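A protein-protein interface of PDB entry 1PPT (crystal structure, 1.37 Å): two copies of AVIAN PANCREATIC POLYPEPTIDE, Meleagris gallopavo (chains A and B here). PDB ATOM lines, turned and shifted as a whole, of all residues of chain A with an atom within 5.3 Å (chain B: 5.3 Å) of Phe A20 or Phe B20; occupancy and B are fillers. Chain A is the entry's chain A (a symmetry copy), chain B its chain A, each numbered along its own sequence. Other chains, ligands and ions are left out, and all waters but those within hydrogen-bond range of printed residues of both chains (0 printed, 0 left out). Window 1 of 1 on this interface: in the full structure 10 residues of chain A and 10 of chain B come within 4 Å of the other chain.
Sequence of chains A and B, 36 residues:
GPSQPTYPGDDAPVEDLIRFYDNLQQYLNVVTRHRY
Tyr A7 touches its own counterpart, Tyr B7.
Phe B20 touches its own counterpart, Phe A20.
Tyr B21 touches its own counterpart, Tyr A21.
Tyr A21 touches Gln B25, and with the chains exchanged Gln A25 touches Tyr B21.
14 positions are printed for both chains.
Of the 5 pairs that touch across the chains among the printed residues, 5 have their exchanged pair printed and touching as well.
Hydrophobic or aromatic side chains of chain B that line the printed part of chain A: Tyr B7, Phe B20 and Tyr B21.
Among the printed residues, no Asp or Glu carboxylate lies within 4 Å of a Lys or Arg side-chain nitrogen of the other chain.
Of the printed residues of chain B, Tyr A7 touches Tyr B7.
Of the printed residues of chain A, Tyr B21 touches Tyr A21 and Gln A25.
Of the printed residues of chain A, Gln B25 touches Tyr A21 (3.0 Å).
The nearest residue of chain B that does not touch Phe A20 is Leu B24 (4.05 Å).
The nearest printed residue of chain B that does not touch Tyr A7 is Phe B20 (4.2 Å).
OH of Tyr B21 lies within hydrogen-bond range of OH of Tyr A21 (3.3 Å).
OH of Tyr B21 lies close to OE1 of Gln A25 (3.0 Å).
The side-chain hydroxyl of Tyr A21 lies close to the side-chain amide oxygen of Gln B25.
CB of Tyr A7 touches CE2 of Tyr B7, 3.9 Å away.
Phe A20 touches Phe B20 (CE1 to CE1, 3.8 Å).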
ATOM      1  N   PRO A   5     -36.754  30.394  -4.177  1.00  0.00           N
ATOM      2  CA  PRO A   5     -36.638  31.091  -5.413  1.00  0.00           C
ATOM      3  C   PRO A   5     -37.418  30.341  -6.553  1.00  0.00           C
ATOM      4  O   PRO A   5     -37.545  29.146  -6.487  1.00  0.00           O
ATOM      5  CB  PRO A   5     -35.189  31.197  -5.805  1.00  0.00           C
ATOM      6  CG  PRO A   5     -34.422  30.667  -4.615  1.00  0.00           C
ATOM      7  CD  PRO A   5     -35.343  30.127  -3.576  1.00  0.00           C
ATOM      8  N   THR A   6     -37.845  31.162  -7.437  1.00  0.00           N
ATOM      9  CA  THR A   6     -38.510  30.686  -8.721  1.00  0.00           C
ATOM     10  C   THR A   6     -37.448  30.267  -9.721  1.00  0.00           C
ATOM     11  O   THR A   6     -36.604  31.061 -10.128  1.00  0.00           O
ATOM     12  CB  THR A   6     -39.361  31.862  -9.212  1.00  0.00           C
ATOM     13  OG1 THR A   6     -40.494  31.682  -8.235  1.00  0.00           O
ATOM     14  CG2 THR A   6     -40.148  31.280 -10.456  1.00  0.00           C
ATOM     15  N   TYR A   7     -37.479  29.026 -10.191  1.00  0.00           N
ATOM     16  CA  TYR A   7     -36.607  28.540 -11.284  1.00  0.00           C
ATOM     17  C   TYR A   7     -36.922  29.286 -12.586  1.00  0.00           C
ATOM     18  O   TYR A   7     -38.084  29.382 -13.006  1.00  0.00           O
ATOM     19  CB  TYR A   7     -36.858  27.038 -11.462  1.00  0.00           C
ATOM     20  CG  TYR A   7     -35.969  26.444 -12.569  1.00  0.00           C
ATOM     21  CD1 TYR A   7     -34.574  26.525 -12.465  1.00  0.00           C
ATOM     22  CD2 TYR A   7     -36.541  25.827 -13.690  1.00  0.00           C
ATOM     23  CE1 TYR A   7     -33.757  25.972 -13.459  1.00  0.00           C
ATOM     24  CE2 TYR A   7     -35.723  25.272 -14.684  1.00  0.00           C
ATOM     25  CZ  TYR A   7     -34.329  25.338 -14.566  1.00  0.00           C
ATOM     26  OH  TYR A   7     -33.528  24.776 -15.510  1.00  0.00           O
ATOM     27  N   PRO A   8     -35.998  29.957 -13.172  1.00  0.00           N
ATOM     28  CA  PRO A   8     -36.187  30.788 -14.390  1.00  0.00           C
ATOM     29  C   PRO A   8     -36.420  30.015 -15.649  1.00  0.00           C
ATOM     30  O   PRO A   8     -36.816  30.691 -16.736  1.00  0.00           O
ATOM     31  CB  PRO A   8     -34.951  31.721 -14.442  1.00  0.00           C
ATOM     32  CG  PRO A   8     -33.887  30.959 -13.795  1.00  0.00           C
ATOM     33  CD  PRO A   8     -34.594  30.071 -12.707  1.00  0.00           C
ATOM     34  N   ASP A  16     -29.199  34.789 -16.007  1.00  0.00           N
ATOM     35  CA  ASP A  16     -30.331  34.391 -15.175  1.00  0.00           C
ATOM     36  C   ASP A  16     -30.140  33.025 -14.533  1.00  0.00           C
ATOM     37  O   ASP A  16     -30.529  32.834 -13.369  1.00  0.00           O
ATOM     38  CB  ASP A  16     -31.654  34.352 -15.877  1.00  0.00           C
ATOM     39  CG  ASP A  16     -32.097  35.730 -16.353  1.00  0.00           C
ATOM     40  OD1 ASP A  16     -33.015  35.833 -17.251  1.00  0.00           O
ATOM     41  OD2 ASP A  16     -31.549  36.785 -15.859  1.00  0.00           O
ATOM     42  N   LEU A  17     -29.461  32.078 -15.051  1.00  0.00           N
ATOM     43  CA  LEU A  17     -29.244  30.872 -14.204  1.00  0.00           C
ATOM     44  C   LEU A  17     -28.177  31.132 -13.143  1.00  0.00           C
ATOM     45  O   LEU A  17     -28.279  30.568 -12.119  1.00  0.00           O
ATOM     46  CB  LEU A  17     -28.583  29.844 -15.161  1.00  0.00           C
ATOM     47  CG  LEU A  17     -29.667  29.275 -16.078  1.00  0.00           C
ATOM     48  CD1 LEU A  17     -28.951  28.342 -17.076  1.00  0.00           C
ATOM     49  CD2 LEU A  17     -30.763  28.509 -15.236  1.00  0.00           C
ATOM     50  N   ILE A  18     -27.237  32.071 -13.335  1.00  0.00           N
ATOM     51  CA  ILE A  18     -26.271  32.467 -12.269  1.00  0.00           C
ATOM     52  C   ILE A  18     -27.058  33.258 -11.202  1.00  0.00           C
ATOM     53  O   ILE A  18     -26.841  32.927 -10.017  1.00  0.00           O
ATOM     54  CB  ILE A  18     -25.189  33.333 -12.920  1.00  0.00           C
ATOM     55  CG1 ILE A  18     -24.236  32.434 -13.755  1.00  0.00           C
ATOM     56  CG2 ILE A  18     -24.464  34.081 -11.795  1.00  0.00           C
ATOM     57  CD1 ILE A  18     -23.299  33.220 -14.529  1.00  0.00           C
ATOM     58  N   ARG A  19     -27.963  34.177 -11.555  1.00  0.00           N
ATOM     59  CA  ARG A  19     -28.778  34.799 -10.436  1.00  0.00           C
ATOM     60  C   ARG A  19     -29.549  33.715  -9.681  1.00  0.00           C
ATOM     61  O   ARG A  19     -29.751  33.807  -8.461  1.00  0.00           O
ATOM     62  CB  ARG A  19     -29.679  35.733 -11.151  1.00  0.00           C
ATOM     63  CG  ARG A  19     -29.198  37.207 -11.068  1.00  0.00           C
ATOM     64  CD  ARG A  19     -30.122  38.315 -11.679  1.00  0.00           C
ATOM     65  NE  ARG A  19     -29.448  38.791 -12.855  1.00  0.00           N
ATOM     66  CZ  ARG A  19     -29.019  39.953 -13.423  1.00  0.00           C
ATOM     67  NH1 ARG A  19     -29.099  41.383 -13.113  1.00  0.00           N
ATOM     68  NH2 ARG A  19     -28.352  39.696 -14.432  1.00  0.00           N
ATOM     69  N   PHE A  20     -30.224  32.765 -10.307  1.00  0.00           N
ATOM     70  CA  PHE A  20     -30.998  31.756  -9.628  1.00  0.00           C
ATOM     71  C   PHE A  20     -30.046  30.953  -8.739  1.00  0.00           C
ATOM     72  O   PHE A  20     -30.378  30.602  -7.599  1.00  0.00           O
ATOM     73  CB  PHE A  20     -31.635  30.832 -10.668  1.00  0.00           C
ATOM     74  CG  PHE A  20     -32.350  29.662 -10.005  1.00  0.00           C
ATOM     75  CD1 PHE A  20     -31.831  28.365 -10.104  1.00  0.00           C
ATOM     76  CD2 PHE A  20     -33.527  29.900  -9.295  1.00  0.00           C
ATOM     77  CE1 PHE A  20     -32.498  27.303  -9.481  1.00  0.00           C
ATOM     78  CE2 PHE A  20     -34.190  28.840  -8.674  1.00  0.00           C
ATOM     79  CZ  PHE A  20     -33.675  27.542  -8.763  1.00  0.00           C
ATOM     80  N   TYR A  21     -28.838  30.558  -9.217  1.00  0.00           N
ATOM     81  CA  TYR A  21     -27.867  29.796  -8.500  1.00  0.00           C
ATOM     82  C   TYR A  21     -27.562  30.520  -7.186  1.00  0.00           C
ATOM     83  O   TYR A  21     -27.567  29.920  -6.106  1.00  0.00           O
ATOM     84  CB  TYR A  21     -26.579  29.708  -9.333  1.00  0.00           C
ATOM     85  CG  TYR A  21     -25.381  29.142  -8.606  1.00  0.00           C
ATOM     86  CD1 TYR A  21     -25.313  27.777  -8.312  1.00  0.00           C
ATOM     87  CD2 TYR A  21     -24.355  30.010  -8.249  1.00  0.00           C
ATOM     88  CE1 TYR A  21     -24.195  27.277  -7.635  1.00  0.00           C
ATOM     89  CE2 TYR A  21     -23.243  29.513  -7.572  1.00  0.00           C
ATOM     90  CZ  TYR A  21     -23.162  28.150  -7.265  1.00  0.00           C
ATOM     91  OH  TYR A  21     -22.073  27.685  -6.595  1.00  0.00           O
ATOM     92  N   ASP A  22     -27.290  31.855  -7.291  1.00  0.00           N
ATOM     93  CA  ASP A  22     -26.934  32.616  -6.062  1.00  0.00           C
ATOM     94  C   ASP A  22     -28.124  32.644  -5.113  1.00  0.00           C
ATOM     95  O   ASP A  22     -27.948  32.579  -3.894  1.00  0.00           O
ATOM     96  CB  ASP A  22     -26.552  34.041  -6.471  1.00  0.00           C
ATOM     97  CG  ASP A  22     -25.196  34.142  -7.150  1.00  0.00           C
ATOM     98  OD1 ASP A  22     -24.956  35.129  -7.937  1.00  0.00           O
ATOM     99  OD2 ASP A  22     -24.294  33.252  -6.934  1.00  0.00           O
ATOM    100  N   ASN A  23     -29.379  32.804  -5.616  1.00  0.00           N
ATOM    101  CA  ASN A  23     -30.508  32.880  -4.684  1.00  0.00           C
ATOM    102  C   ASN A  23     -30.719  31.448  -4.128  1.00  0.00           C
ATOM    103  O   ASN A  23     -31.088  31.383  -2.925  1.00  0.00           O
ATOM    104  CB  ASN A  23     -31.757  33.378  -5.362  1.00  0.00           C
ATOM    105  CG  ASN A  23     -31.718  34.867  -5.713  1.00  0.00           C
ATOM    106  OD1 ASN A  23     -32.691  35.220  -6.565  1.00  0.00           O
ATOM    107  ND2 ASN A  23     -30.899  35.648  -5.241  1.00  0.00           N
ATOM    108  N   LEU A  24     -30.534  30.410  -4.888  1.00  0.00           N
ATOM    109  CA  LEU A  24     -30.767  29.017  -4.256  1.00  0.00           C
ATOM    110  C   LEU A  24     -29.682  28.827  -3.163  1.00  0.00           C
ATOM    111  O   LEU A  24     -30.006  28.171  -2.233  1.00  0.00           O
ATOM    112  CB  LEU A  24     -30.526  28.070  -5.400  1.00  0.00           C
ATOM    113  CG  LEU A  24     -30.798  26.605  -5.018  1.00  0.00           C
ATOM    114  CD1 LEU A  24     -32.170  26.458  -4.477  1.00  0.00           C
ATOM    115  CD2 LEU A  24     -30.580  25.641  -6.251  1.00  0.00           C
ATOM    116  N   GLN A  25     -28.455  29.289  -3.360  1.00  0.00           N
ATOM    117  CA  GLN A  25     -27.413  29.183  -2.389  1.00  0.00           C
ATOM    118  C   GLN A  25     -27.832  29.833  -1.072  1.00  0.00           C
ATOM    119  O   GLN A  25     -27.793  29.191  -0.011  1.00  0.00           O
ATOM    120  CB  GLN A  25     -26.118  29.840  -2.860  1.00  0.00           C
ATOM    121  CG  GLN A  25     -24.929  29.669  -1.921  1.00  0.00           C
ATOM    122  CD  GLN A  25     -23.590  29.897  -2.635  1.00  0.00           C
ATOM    123  OE1 GLN A  25     -22.545  29.503  -2.116  1.00  0.00           O
ATOM    124  NE2 GLN A  25     -23.560  30.510  -3.805  1.00  0.00           N
ATOM    125  N   PRO B   5     -28.601  20.278 -16.143  1.00  0.00           N
ATOM    126  CA  PRO B   5     -29.284  19.465 -15.194  1.00  0.00           C
ATOM    127  C   PRO B   5     -30.831  19.737 -15.236  1.00  0.00           C
ATOM    128  O   PRO B   5     -31.227  20.824 -15.566  1.00  0.00           O
ATOM    129  CB  PRO B   5     -28.776  19.761 -13.809  1.00  0.00           C
ATOM    130  CG  PRO B   5     -27.602  20.690 -14.013  1.00  0.00           C
ATOM    131  CD  PRO B   5     -27.456  21.070 -15.446  1.00  0.00           C
ATOM    132  N   THR B   6     -31.492  18.692 -14.903  1.00  0.00           N
ATOM    133  CA  THR B   6     -33.004  18.721 -14.724  1.00  0.00           C
ATOM    134  C   THR B   6     -33.345  19.288 -13.359  1.00  0.00           C
ATOM    135  O   THR B   6     -32.958  18.747 -12.326  1.00  0.00           O
ATOM    136  CB  THR B   6     -33.474  17.273 -14.904  1.00  0.00           C
ATOM    137  OG1 THR B   6     -33.377  17.240 -16.408  1.00  0.00           O
ATOM    138  CG2 THR B   6     -35.053  17.368 -14.862  1.00  0.00           C
ATOM    139  N   TYR B   7     -34.121  20.363 -13.299  1.00  0.00           N
ATOM    140  CA  TYR B   7     -34.659  20.917 -12.036  1.00  0.00           C
ATOM    141  C   TYR B   7     -35.610  19.912 -11.376  1.00  0.00           C
ATOM    142  O   TYR B   7     -36.533  19.387 -12.015  1.00  0.00           O
ATOM    143  CB  TYR B   7     -35.408  22.213 -12.365  1.00  0.00           C
ATOM    144  CG  TYR B   7     -35.982  22.873 -11.098  1.00  0.00           C
ATOM    145  CD1 TYR B   7     -35.123  23.255 -10.058  1.00  0.00           C
ATOM    146  CD2 TYR B   7     -37.361  23.089 -10.967  1.00  0.00           C
ATOM    147  CE1 TYR B   7     -35.634  23.871  -8.909  1.00  0.00           C
ATOM    148  CE2 TYR B   7     -37.872  23.707  -9.817  1.00  0.00           C
ATOM    149  CZ  TYR B   7     -37.008  24.105  -8.790  1.00  0.00           C
ATOM    150  OH  TYR B   7     -37.491  24.732  -7.685  1.00  0.00           O
ATOM    151  N   PRO B   8     -35.358  19.482 -10.193  1.00  0.00           N
ATOM    152  CA  PRO B   8     -36.148  18.450  -9.472  1.00  0.00           C
ATOM    153  C   PRO B   8     -37.501  18.897  -9.018  1.00  0.00           C
ATOM    154  O   PRO B   8     -38.350  17.965  -8.563  1.00  0.00           O
ATOM    155  CB  PRO B   8     -35.228  17.960  -8.326  1.00  0.00           C
ATOM    156  CG  PRO B   8     -34.390  19.113  -8.008  1.00  0.00           C
ATOM    157  CD  PRO B   8     -34.202  19.895  -9.359  1.00  0.00           C
ATOM    158  N   ASP B  16     -32.382  16.659  -2.397  1.00  0.00           N
ATOM    159  CA  ASP B  16     -32.468  16.807  -3.847  1.00  0.00           C
ATOM    160  C   ASP B  16     -32.295  18.247  -4.304  1.00  0.00           C
ATOM    161  O   ASP B  16     -31.656  18.490  -5.342  1.00  0.00           O
ATOM    162  CB  ASP B  16     -33.741  16.312  -4.463  1.00  0.00           C
ATOM    163  CG  ASP B  16     -33.916  14.807  -4.300  1.00  0.00           C
ATOM    164  OD1 ASP B  16     -35.079  14.277  -4.458  1.00  0.00           O
ATOM    165  OD2 ASP B  16     -32.901  14.073  -4.001  1.00  0.00           O
ATOM    166  N   LEU B  17     -32.634  19.265  -3.613  1.00  0.00           N
ATOM    167  CA  LEU B  17     -32.236  20.597  -4.148  1.00  0.00           C
ATOM    168  C   LEU B  17     -30.751  20.861  -3.914  1.00  0.00           C
ATOM    169  O   LEU B  17     -30.184  21.521  -4.702  1.00  0.00           O
ATOM    170  CB  LEU B  17     -32.953  21.613  -3.220  1.00  0.00           C
ATOM    171  CG  LEU B  17     -34.432  21.655  -3.604  1.00  0.00           C
ATOM    172  CD1 LEU B  17     -35.122  22.594  -2.592  1.00  0.00           C
ATOM    173  CD2 LEU B  17     -34.608  22.160  -5.091  1.00  0.00           C
ATOM    174  N   ILE B  18     -30.098  20.249  -2.913  1.00  0.00           N
ATOM    175  CA  ILE B  18     -28.620  20.356  -2.739  1.00  0.00           C
ATOM    176  C   ILE B  18     -27.960  19.538  -3.870  1.00  0.00           C
ATOM    177  O   ILE B  18     -27.022  20.107  -4.469  1.00  0.00           O
ATOM    178  CB  ILE B  18     -28.271  19.784  -1.361  1.00  0.00           C
ATOM    179  CG1 ILE B  18     -28.694  20.792  -0.257  1.00  0.00           C
ATOM    180  CG2 ILE B  18     -26.766  19.494  -1.355  1.00  0.00           C
ATOM    181  CD1 ILE B  18     -28.545  20.229   1.067  1.00  0.00           C
ATOM    182  N   ARG B  19     -28.433  18.336  -4.217  1.00  0.00           N
ATOM    183  CA  ARG B  19     -27.801  17.677  -5.429  1.00  0.00           C
ATOM    184  C   ARG B  19     -27.970  18.568  -6.661  1.00  0.00           C
ATOM    185  O   ARG B  19     -27.096  18.613  -7.539  1.00  0.00           O
ATOM    186  CB  ARG B  19     -28.549  16.404  -5.550  1.00  0.00           C
ATOM    187  CG  ARG B  19     -27.759  15.191  -4.989  1.00  0.00           C
ATOM    188  CD  ARG B  19     -28.383  13.765  -5.163  1.00  0.00           C
ATOM    189  NE  ARG B  19     -28.789  13.344  -3.851  1.00  0.00           N
ATOM    190  CZ  ARG B  19     -28.634  12.302  -2.987  1.00  0.00           C
ATOM    191  NH1 ARG B  19     -27.983  10.989  -3.007  1.00  0.00           N
ATOM    192  NH2 ARG B  19     -29.144  12.591  -1.898  1.00  0.00           N
ATOM    193  N   PHE B  20     -29.123  19.142  -6.962  1.00  0.00           N
ATOM    194  CA  PHE B  20     -29.328  19.950  -8.138  1.00  0.00           C
ATOM    195  C   PHE B  20     -28.375  21.145  -8.060  1.00  0.00           C
ATOM    196  O   PHE B  20     -27.775  21.551  -9.064  1.00  0.00           O
ATOM    197  CB  PHE B  20     -30.775  20.446  -8.156  1.00  0.00           C
ATOM    198  CG  PHE B  20     -31.013  21.420  -9.303  1.00  0.00           C
ATOM    199  CD1 PHE B  20     -31.221  22.781  -9.046  1.00  0.00           C
ATOM    200  CD2 PHE B  20     -31.017  20.939 -10.613  1.00  0.00           C
ATOM    201  CE1 PHE B  20     -31.429  23.663 -10.113  1.00  0.00           C
ATOM    202  CE2 PHE B  20     -31.223  21.820 -11.675  1.00  0.00           C
ATOM    203  CZ  PHE B  20     -31.426  23.182 -11.427  1.00  0.00           C
ATOM    204  N   TYR B  21     -28.222  21.819  -6.892  1.00  0.00           N
ATOM    205  CA  TYR B  21     -27.380  22.953  -6.689  1.00  0.00           C
ATOM    206  C   TYR B  21     -25.961  22.583  -7.128  1.00  0.00           C
ATOM    207  O   TYR B  21     -25.309  23.317  -7.879  1.00  0.00           O
ATOM    208  CB  TYR B  21     -27.365  23.309  -5.194  1.00  0.00           C
ATOM    209  CG  TYR B  21     -26.331  24.334  -4.788  1.00  0.00           C
ATOM    210  CD1 TYR B  21     -26.496  25.679  -5.132  1.00  0.00           C
ATOM    211  CD2 TYR B  21     -25.225  23.904  -4.063  1.00  0.00           C
ATOM    212  CE1 TYR B  21     -25.523  26.609  -4.747  1.00  0.00           C
ATOM    213  CE2 TYR B  21     -24.255  24.829  -3.682  1.00  0.00           C
ATOM    214  CZ  TYR B  21     -24.402  26.178  -4.024  1.00  0.00           C
ATOM    215  OH  TYR B  21     -23.439  27.066  -3.652  1.00  0.00           O
ATOM    216  N   ASP B  22     -25.474  21.405  -6.637  1.00  0.00           N
ATOM    217  CA  ASP B  22     -24.082  21.003  -6.979  1.00  0.00           C
ATOM    218  C   ASP B  22     -23.973  20.753  -8.476  1.00  0.00           C
ATOM    219  O   ASP B  22     -22.947  21.064  -9.085  1.00  0.00           O
ATOM    220  CB  ASP B  22     -23.745  19.726  -6.205  1.00  0.00           C
ATOM    221  CG  ASP B  22     -23.513  19.951  -4.720  1.00  0.00           C
ATOM    222  OD1 ASP B  22     -23.687  18.978  -3.899  1.00  0.00           O
ATOM    223  OD2 ASP B  22     -23.140  21.103  -4.289  1.00  0.00           O
ATOM    224  N   ASN B  23     -24.991  20.126  -9.128  1.00  0.00           N
ATOM    225  CA  ASN B  23     -24.848  19.847 -10.560  1.00  0.00           C
ATOM    226  C   ASN B  23     -24.979  21.209 -11.290  1.00  0.00           C
ATOM    227  O   ASN B  23     -24.259  21.345 -12.315  1.00  0.00           O
ATOM    228  CB  ASN B  23     -25.892  18.878 -11.045  1.00  0.00           C
ATOM    229  CG  ASN B  23     -25.675  17.441 -10.564  1.00  0.00           C
ATOM    230  OD1 ASN B  23     -26.752  16.668 -10.754  1.00  0.00           O
ATOM    231  ND2 ASN B  23     -24.617  17.046 -10.084  1.00  0.00           N
ATOM    232  N   LEU B  24     -25.801  22.116 -10.853  1.00  0.00           N
ATOM    233  CA  LEU B  24     -25.874  23.446 -11.640  1.00  0.00           C
ATOM    234  C   LEU B  24     -24.496  24.142 -11.483  1.00  0.00           C
ATOM    235  O   LEU B  24     -24.152  24.802 -12.403  1.00  0.00           O
ATOM    236  CB  LEU B  24     -26.937  24.224 -10.914  1.00  0.00           C
ATOM    237  CG  LEU B  24     -27.249  25.569 -11.591  1.00  0.00           C
ATOM    238  CD1 LEU B  24     -27.612  25.359 -13.013  1.00  0.00           C
ATOM    239  CD2 LEU B  24     -28.399  26.342 -10.831  1.00  0.00           C
ATOM    240  N   GLN B  25     -23.843  24.066 -10.332  1.00  0.00           N
ATOM    241  CA  GLN B  25     -22.557  24.651 -10.121  1.00  0.00           C
ATOM    242  C   GLN B  25     -21.549  24.122 -11.139  1.00  0.00           C
ATOM    243  O   GLN B  25     -20.902  24.905 -11.852  1.00  0.00           O
ATOM    244  CB  GLN B  25     -22.019  24.371  -8.720  1.00  0.00           C
ATOM    245  CG  GLN B  25     -20.700  25.058  -8.385  1.00  0.00           C
ATOM    246  CD  GLN B  25     -20.464  25.153  -6.872  1.00  0.00           C
ATOM    247  OE1 GLN B  25     -19.621  25.935  -6.433  1.00  0.00           O
ATOM    248  NE2 GLN B  25     -21.168  24.401  -6.044  1.00  0.00           N
